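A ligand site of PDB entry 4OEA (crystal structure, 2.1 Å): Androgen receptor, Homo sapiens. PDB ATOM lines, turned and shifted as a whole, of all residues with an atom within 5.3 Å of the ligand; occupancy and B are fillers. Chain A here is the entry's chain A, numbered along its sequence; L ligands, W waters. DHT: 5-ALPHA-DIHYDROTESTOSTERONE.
Water W1 lies within hydrogen-bond range of NE2 of Gln 42, O of Met 76, NH2 of Arg 83 and O3 of the ligand.
The guanidinium group (NH2) of Arg 83 is in hydrogen-bond range of the side-chain amide oxygen (OE1) of Gln 42. The side-chain amide nitrogen (ND2) of Asn 36 sits close to the backbone carbonyl oxygen (O) of Leu 32 (3.4 Å). The guanidinium group (NH2) of Arg 83 lies within hydrogen-bond range of the backbone carbonyl oxygen (O) of Phe 95 (2.9 Å).
Merely in contact with the ligand: Leu 32 (3.8 Å), Leu 35 (3.4 Å), Gln 42 (3.4 Å), Met 73 (3.9 Å), Met 76 (3.7 Å), Met 80 (3.6 Å), Phe 95 (3.6 Å), Met 111 (3.9 Å), Phe 207 (3.8 Å), Phe 222 (3.9 Å) and Met 226 (3.8 Å). 14 residues have an atom within 4 Å of the ligand: Leu 32, Leu 35, Asn 36, Gln 42, Met 73, Met 76, Met 80, Arg 83, Phe 95, Met 111, Phe 207, Thr 208, Phe 222 and Met 226.
An oxygen (O17) of the ligand lies within hydrogen-bond range of the side-chain hydroxyl of Thr 208 (2.7 Å). The side-chain amide oxygen (OD1) of Asn 36 lies within hydrogen-bond range of an oxygen (O17) of the ligand. The guanidinium group (NH2) of Arg 83 is in hydrogen-bond range of an oxygen (O3) of the ligand, at 3.0 Å.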
ATOM      1  N   LEU A  32      23.184  33.547 -14.653  1.00  0.00           N
ATOM      2  CA  LEU A  32      23.782  32.292 -15.042  1.00  0.00           C
ATOM      3  C   LEU A  32      23.130  31.079 -14.443  1.00  0.00           C
ATOM      4  O   LEU A  32      22.987  30.060 -15.129  1.00  0.00           O
ATOM      5  CB  LEU A  32      25.282  32.345 -14.813  1.00  0.00           C
ATOM      6  CG  LEU A  32      26.102  32.873 -16.002  1.00  0.00           C
ATOM      7  CD1 LEU A  32      26.082  31.912 -17.204  1.00  0.00           C
ATOM      8  CD2 LEU A  32      25.655  34.270 -16.407  1.00  0.00           C
ATOM      9  N   LEU A  35      20.062  30.610 -16.417  1.00  0.00           N
ATOM     10  CA  LEU A  35      20.433  29.999 -17.718  1.00  0.00           C
ATOM     11  C   LEU A  35      20.748  28.531 -17.564  1.00  0.00           C
ATOM     12  O   LEU A  35      20.319  27.723 -18.340  1.00  0.00           O
ATOM     13  CB  LEU A  35      21.648  30.712 -18.320  1.00  0.00           C
ATOM     14  CG  LEU A  35      21.393  32.055 -19.023  1.00  0.00           C
ATOM     15  CD1 LEU A  35      22.731  32.599 -19.473  1.00  0.00           C
ATOM     16  CD2 LEU A  35      20.417  31.933 -20.184  1.00  0.00           C
ATOM     17  N   ASN A  36      21.485  28.215 -16.500  1.00  0.00           N
ATOM     18  CA  ASN A  36      21.759  26.818 -16.173  1.00  0.00           C
ATOM     19  C   ASN A  36      20.522  25.989 -15.935  1.00  0.00           C
ATOM     20  O   ASN A  36      20.422  24.823 -16.388  1.00  0.00           O
ATOM     21  CB  ASN A  36      22.689  26.752 -14.947  1.00  0.00           C
ATOM     22  CG  ASN A  36      24.103  27.134 -15.290  1.00  0.00           C
ATOM     23  OD1 ASN A  36      24.473  27.172 -16.481  1.00  0.00           O
ATOM     24  ND2 ASN A  36      24.920  27.437 -14.256  1.00  0.00           N
ATOM     25  N   LEU A  38      17.499  26.727 -17.099  1.00  0.00           N
ATOM     26  CA  LEU A  38      16.867  26.670 -18.426  1.00  0.00           C
ATOM     27  C   LEU A  38      17.496  25.577 -19.268  1.00  0.00           C
ATOM     28  O   LEU A  38      16.802  24.860 -19.977  1.00  0.00           O
ATOM     29  CB  LEU A  38      17.011  28.034 -19.191  1.00  0.00           C
ATOM     30  CG  LEU A  38      16.299  28.054 -20.565  1.00  0.00           C
ATOM     31  CD1 LEU A  38      14.798  27.825 -20.445  1.00  0.00           C
ATOM     32  CD2 LEU A  38      16.536  29.358 -21.263  1.00  0.00           C
ATOM     33  N   GLY A  39      18.797  25.427 -19.158  1.00  0.00           N
ATOM     34  CA  GLY A  39      19.480  24.366 -19.860  1.00  0.00           C
ATOM     35  C   GLY A  39      19.030  22.981 -19.414  1.00  0.00           C
ATOM     36  O   GLY A  39      18.810  22.087 -20.225  1.00  0.00           O
ATOM     37  N   GLN A  42      15.408  22.542 -20.796  1.00  0.00           N
ATOM     38  CA  GLN A  42      15.412  22.337 -22.245  1.00  0.00           C
ATOM     39  C   GLN A  42      16.025  21.008 -22.635  1.00  0.00           C
ATOM     40  O   GLN A  42      15.662  20.414 -23.627  1.00  0.00           O
ATOM     41  CB  GLN A  42      16.101  23.506 -22.951  1.00  0.00           C
ATOM     42  CG  GLN A  42      15.242  24.756 -22.989  1.00  0.00           C
ATOM     43  CD  GLN A  42      15.763  25.815 -23.933  1.00  0.00           C
ATOM     44  OE1 GLN A  42      15.374  26.991 -23.851  1.00  0.00           O
ATOM     45  NE2 GLN A  42      16.655  25.425 -24.832  1.00  0.00           N
ATOM     46  N   TRP A  72      23.773  19.316 -27.892  1.00  0.00           N
ATOM     47  CA  TRP A  72      22.792  20.082 -27.213  1.00  0.00           C
ATOM     48  C   TRP A  72      23.058  21.559 -27.212  1.00  0.00           C
ATOM     49  O   TRP A  72      22.125  22.303 -27.322  1.00  0.00           O
ATOM     50  CB  TRP A  72      22.578  19.644 -25.731  1.00  0.00           C
ATOM     51  CG  TRP A  72      23.784  19.770 -24.850  1.00  0.00           C
ATOM     52  CD1 TRP A  72      24.742  18.843 -24.667  1.00  0.00           C
ATOM     53  CD2 TRP A  72      24.145  20.891 -24.035  1.00  0.00           C
ATOM     54  NE1 TRP A  72      25.715  19.313 -23.788  1.00  0.00           N
ATOM     55  CE2 TRP A  72      25.342  20.561 -23.375  1.00  0.00           C
ATOM     56  CE3 TRP A  72      23.550  22.121 -23.767  1.00  0.00           C
ATOM     57  CZ2 TRP A  72      25.966  21.444 -22.496  1.00  0.00           C
ATOM     58  CZ3 TRP A  72      24.169  22.980 -22.888  1.00  0.00           C
ATOM     59  CH2 TRP A  72      25.363  22.643 -22.265  1.00  0.00           C
ATOM     60  N   MET A  73      24.307  21.998 -27.044  1.00  0.00           N
ATOM     61  CA  MET A  73      24.603  23.422 -27.032  1.00  0.00           C
ATOM     62  C   MET A  73      24.212  24.084 -28.365  1.00  0.00           C
ATOM     63  O   MET A  73      23.558  25.100 -28.364  1.00  0.00           O
ATOM     64  CB  MET A  73      26.090  23.670 -26.769  1.00  0.00           C
ATOM     65  CG  MET A  73      26.454  25.117 -26.565  1.00  0.00           C
ATOM     66  SD  MET A  73      25.827  25.852 -25.038  1.00  0.00           S
ATOM     67  CE  MET A  73      27.041  25.168 -23.921  1.00  0.00           C
ATOM     68  N   MET A  76      20.322  24.099 -28.896  1.00  0.00           N
ATOM     69  CA  MET A  76      19.636  25.109 -28.107  1.00  0.00           C
ATOM     70  C   MET A  76      19.938  26.570 -28.562  1.00  0.00           C
ATOM     71  O   MET A  76      19.084  27.449 -28.495  1.00  0.00           O
ATOM     72  CB  MET A  76      20.032  24.943 -26.645  1.00  0.00           C
ATOM     73  CG  MET A  76      19.557  23.558 -26.035  1.00  0.00           C
ATOM     74  SD  MET A  76      19.952  23.544 -24.304  1.00  0.00           S
ATOM     75  CE  MET A  76      19.472  21.829 -23.967  1.00  0.00           C
ATOM     76  N   VAL A  77      21.176  26.818 -28.935  1.00  0.00           N
ATOM     77  CA  VAL A  77      21.586  28.137 -29.436  1.00  0.00           C
ATOM     78  C   VAL A  77      20.845  28.495 -30.725  1.00  0.00           C
ATOM     79  O   VAL A  77      20.411  29.609 -30.862  1.00  0.00           O
ATOM     80  CB  VAL A  77      23.103  28.250 -29.642  1.00  0.00           C
ATOM     81  CG1 VAL A  77      23.478  29.548 -30.420  1.00  0.00           C
ATOM     82  CG2 VAL A  77      23.831  28.227 -28.301  1.00  0.00           C
ATOM     83  N   MET A  80      17.278  29.156 -29.945  1.00  0.00           N
ATOM     84  CA  MET A  80      17.170  30.418 -29.275  1.00  0.00           C
ATOM     85  C   MET A  80      17.294  31.597 -30.269  1.00  0.00           C
ATOM     86  O   MET A  80      16.598  32.609 -30.130  1.00  0.00           O
ATOM     87  CB  MET A  80      18.214  30.525 -28.193  1.00  0.00           C
ATOM     88  CG  MET A  80      18.097  31.782 -27.339  1.00  0.00           C
ATOM     89  SD  MET A  80      18.936  33.263 -27.946  1.00  0.00           S
ATOM     90  CE  MET A  80      20.646  32.817 -27.964  1.00  0.00           C
ATOM     91  N   ARG A  83      13.962  31.894 -31.922  1.00  0.00           N
ATOM     92  CA  ARG A  83      13.005  32.551 -31.004  1.00  0.00           C
ATOM     93  C   ARG A  83      13.252  34.035 -30.957  1.00  0.00           C
ATOM     94  O   ARG A  83      12.312  34.804 -30.924  1.00  0.00           O
ATOM     95  CB  ARG A  83      13.131  32.000 -29.573  1.00  0.00           C
ATOM     96  CG  ARG A  83      12.589  30.615 -29.386  1.00  0.00           C
ATOM     97  CD  ARG A  83      12.304  30.285 -27.914  1.00  0.00           C
ATOM     98  NE  ARG A  83      13.534  30.277 -27.148  1.00  0.00           N
ATOM     99  CZ  ARG A  83      14.416  29.282 -27.112  1.00  0.00           C
ATOM    100  NH1 ARG A  83      14.241  28.171 -27.811  1.00  0.00           N
ATOM    101  NH2 ARG A  83      15.510  29.403 -26.363  1.00  0.00           N
ATOM    102  N   PHE A  95      15.972  33.885 -24.639  1.00  0.00           N
ATOM    103  CA  PHE A  95      16.291  32.587 -24.076  1.00  0.00           C
ATOM    104  C   PHE A  95      15.020  31.851 -23.610  1.00  0.00           C
ATOM    105  O   PHE A  95      14.851  30.683 -23.893  1.00  0.00           O
ATOM    106  CB  PHE A  95      17.259  32.753 -22.918  1.00  0.00           C
ATOM    107  CG  PHE A  95      18.643  33.134 -23.329  1.00  0.00           C
ATOM    108  CD1 PHE A  95      19.104  34.424 -23.092  1.00  0.00           C
ATOM    109  CD2 PHE A  95      19.504  32.206 -23.893  1.00  0.00           C
ATOM    110  CE1 PHE A  95      20.411  34.755 -23.410  1.00  0.00           C
ATOM    111  CE2 PHE A  95      20.792  32.538 -24.223  1.00  0.00           C
ATOM    112  CZ  PHE A  95      21.252  33.824 -23.976  1.00  0.00           C
ATOM    113  N   MET A 111      29.267  37.504 -20.700  1.00  0.00           N
ATOM    114  CA  MET A 111      29.244  36.729 -21.917  1.00  0.00           C
ATOM    115  C   MET A 111      28.877  37.605 -23.084  1.00  0.00           C
ATOM    116  O   MET A 111      28.260  37.120 -24.044  1.00  0.00           O
ATOM    117  CB  MET A 111      28.144  35.685 -21.822  1.00  0.00           C
ATOM    118  CG  MET A 111      28.367  34.560 -20.867  1.00  0.00           C
ATOM    119  SD  MET A 111      27.305  33.193 -21.447  1.00  0.00           S
ATOM    120  CE  MET A 111      25.706  33.860 -21.045  1.00  0.00           C
ATOM    121  N   MET A 118      25.676  35.296 -30.905  1.00  0.00           N
ATOM    122  CA  MET A 118      24.350  34.659 -30.926  1.00  0.00           C
ATOM    123  C   MET A 118      23.288  35.598 -31.507  1.00  0.00           C
ATOM    124  O   MET A 118      22.361  35.161 -32.203  1.00  0.00           O
ATOM    125  CB  MET A 118      23.947  34.186 -29.507  1.00  0.00           C
ATOM    126  CG  MET A 118      24.772  32.997 -29.013  1.00  0.00           C
ATOM    127  SD  MET A 118      24.090  32.336 -27.490  1.00  0.00           S
ATOM    128  CE  MET A 118      24.696  33.525 -26.296  1.00  0.00           C
ATOM    129  N   LEU A 204      30.870  28.755 -25.942  1.00  0.00           N
ATOM    130  CA  LEU A 204      29.958  28.498 -24.835  1.00  0.00           C
ATOM    131  C   LEU A 204      30.342  27.261 -24.041  1.00  0.00           C
ATOM    132  O   LEU A 204      30.130  27.208 -22.846  1.00  0.00           O
ATOM    133  CB  LEU A 204      28.525  28.404 -25.365  1.00  0.00           C
ATOM    134  CG  LEU A 204      27.985  29.724 -25.933  1.00  0.00           C
ATOM    135  CD1 LEU A 204      26.666  29.500 -26.635  1.00  0.00           C
ATOM    136  CD2 LEU A 204      27.856  30.814 -24.858  1.00  0.00           C
ATOM    137  N   PHE A 207      33.251  28.513 -21.973  1.00  0.00           N
ATOM    138  CA  PHE A 207      32.731  29.405 -20.917  1.00  0.00           C
ATOM    139  C   PHE A 207      32.034  28.627 -19.801  1.00  0.00           C
ATOM    140  O   PHE A 207      32.317  28.844 -18.613  1.00  0.00           O
ATOM    141  CB  PHE A 207      31.778  30.437 -21.514  1.00  0.00           C
ATOM    142  CG  PHE A 207      31.314  31.463 -20.525  1.00  0.00           C
ATOM    143  CD1 PHE A 207      30.157  31.267 -19.759  1.00  0.00           C
ATOM    144  CD2 PHE A 207      32.016  32.656 -20.381  1.00  0.00           C
ATOM    145  CE1 PHE A 207      29.740  32.230 -18.851  1.00  0.00           C
ATOM    146  CE2 PHE A 207      31.596  33.627 -19.469  1.00  0.00           C
ATOM    147  CZ  PHE A 207      30.456  33.407 -18.714  1.00  0.00           C
ATOM    148  N   THR A 208      31.129  27.720 -20.182  1.00  0.00           N
ATOM    149  CA  THR A 208      30.346  26.969 -19.203  1.00  0.00           C
ATOM    150  C   THR A 208      31.202  25.966 -18.423  1.00  0.00           C
ATOM    151  O   THR A 208      30.932  25.654 -17.263  1.00  0.00           O
ATOM    152  CB  THR A 208      29.137  26.241 -19.843  1.00  0.00           C
ATOM    153  OG1 THR A 208      28.232  25.810 -18.825  1.00  0.00           O
ATOM    154  CG2 THR A 208      29.537  25.034 -20.665  1.00  0.00           C
ATOM    155  N   LEU A 211      33.218  28.059 -15.999  1.00  0.00           N
ATOM    156  CA  LEU A 211      32.285  28.512 -14.986  1.00  0.00           C
ATOM    157  C   LEU A 211      31.942  27.397 -13.989  1.00  0.00           C
ATOM    158  O   LEU A 211      31.812  27.655 -12.789  1.00  0.00           O
ATOM    159  CB  LEU A 211      31.018  29.056 -15.664  1.00  0.00           C
ATOM    160  CG  LEU A 211      29.879  29.550 -14.768  1.00  0.00           C
ATOM    161  CD1 LEU A 211      30.395  30.553 -13.743  1.00  0.00           C
ATOM    162  CD2 LEU A 211      28.792  30.163 -15.622  1.00  0.00           C
ATOM    163  N   PHE A 222      24.686  24.990 -10.698  1.00  0.00           N
ATOM    164  CA  PHE A 222      24.574  24.036 -11.794  1.00  0.00           C
ATOM    165  C   PHE A 222      23.686  22.885 -11.403  1.00  0.00           C
ATOM    166  O   PHE A 222      23.994  22.205 -10.436  1.00  0.00           O
ATOM    167  CB  PHE A 222      25.953  23.492 -12.199  1.00  0.00           C
ATOM    168  CG  PHE A 222      26.721  24.423 -13.108  1.00  0.00           C
ATOM    169  CD1 PHE A 222      27.473  25.473 -12.584  1.00  0.00           C
ATOM    170  CD2 PHE A 222      26.662  24.269 -14.483  1.00  0.00           C
ATOM    171  CE1 PHE A 222      28.163  26.353 -13.400  1.00  0.00           C
ATOM    172  CE2 PHE A 222      27.366  25.151 -15.319  1.00  0.00           C
ATOM    173  CZ  PHE A 222      28.107  26.191 -14.779  1.00  0.00           C
ATOM    174  N   MET A 226      23.228  19.052 -16.135  1.00  0.00           N
ATOM    175  CA  MET A 226      24.177  20.048 -16.648  1.00  0.00           C
ATOM    176  C   MET A 226      25.573  19.836 -16.085  1.00  0.00           C
ATOM    177  O   MET A 226      26.538  19.833 -16.823  1.00  0.00           O
ATOM    178  CB  MET A 226      23.685  21.450 -16.326  1.00  0.00           C
ATOM    179  CG  MET A 226      22.427  21.839 -17.130  1.00  0.00           C
ATOM    180  SD  MET A 226      22.703  22.158 -18.915  1.00  0.00           S
ATOM    181  CE  MET A 226      23.442  23.760 -18.735  1.00  0.00           C
ATOM    182  N   ILE A 230      28.596  18.733 -18.594  1.00  0.00           N
ATOM    183  CA  ILE A 230      29.664  19.705 -18.723  1.00  0.00           C
ATOM    184  C   ILE A 230      31.012  19.173 -18.178  1.00  0.00           C
ATOM    185  O   ILE A 230      32.076  19.625 -18.612  1.00  0.00           O
ATOM    186  CB  ILE A 230      29.265  21.065 -18.095  1.00  0.00           C
ATOM    187  CG1 ILE A 230      28.036  21.659 -18.813  1.00  0.00           C
ATOM    188  CG2 ILE A 230      30.419  22.062 -18.152  1.00  0.00           C
ATOM    189  CD1 ILE A 230      27.280  22.711 -18.031  1.00  0.00           C
HETATM  190  C1  DHT L   1      20.136  27.637 -22.426  1.00  0.00           C
HETATM  191  C2  DHT L   1      19.141  27.310 -23.539  1.00  0.00           C
HETATM  192  C3  DHT L   1      19.178  28.438 -24.574  1.00  0.00           C
HETATM  193  O3  DHT L   1      18.123  29.016 -24.945  1.00  0.00           O
HETATM  194  C4  DHT L   1      20.551  28.848 -25.083  1.00  0.00           C
HETATM  195  C5  DHT L   1      21.524  29.034 -23.915  1.00  0.00           C
HETATM  196  C6  DHT L   1      22.894  29.378 -24.454  1.00  0.00           C
HETATM  197  C7  DHT L   1      23.894  29.688 -23.349  1.00  0.00           C
HETATM  198  C8  DHT L   1      23.965  28.552 -22.333  1.00  0.00           C
HETATM  199  C9  DHT L   1      22.570  28.146 -21.823  1.00  0.00           C
HETATM  200  C10 DHT L   1      21.583  27.838 -22.949  1.00  0.00           C
HETATM  201  C11 DHT L   1      22.684  27.045 -20.733  1.00  0.00           C
HETATM  202  C12 DHT L   1      23.582  27.462 -19.575  1.00  0.00           C
HETATM  203  C13 DHT L   1      24.973  27.872 -20.071  1.00  0.00           C
HETATM  204  C14 DHT L   1      24.814  28.971 -21.133  1.00  0.00           C
HETATM  205  C15 DHT L   1      26.246  29.457 -21.394  1.00  0.00           C
HETATM  206  C16 DHT L   1      26.924  29.326 -19.995  1.00  0.00           C
HETATM  207  C17 DHT L   1      25.889  28.605 -19.086  1.00  0.00           C
HETATM  208  O17 DHT L   1      26.476  27.726 -18.136  1.00  0.00           O
HETATM  209  C18 DHT L   1      25.696  26.623 -20.604  1.00  0.00           C
HETATM  210  C19 DHT L   1      22.003  26.537 -23.648  1.00  0.00           C
HETATM  211  O   HOH W   1      16.728  26.760 -26.927  1.00  0.00           O
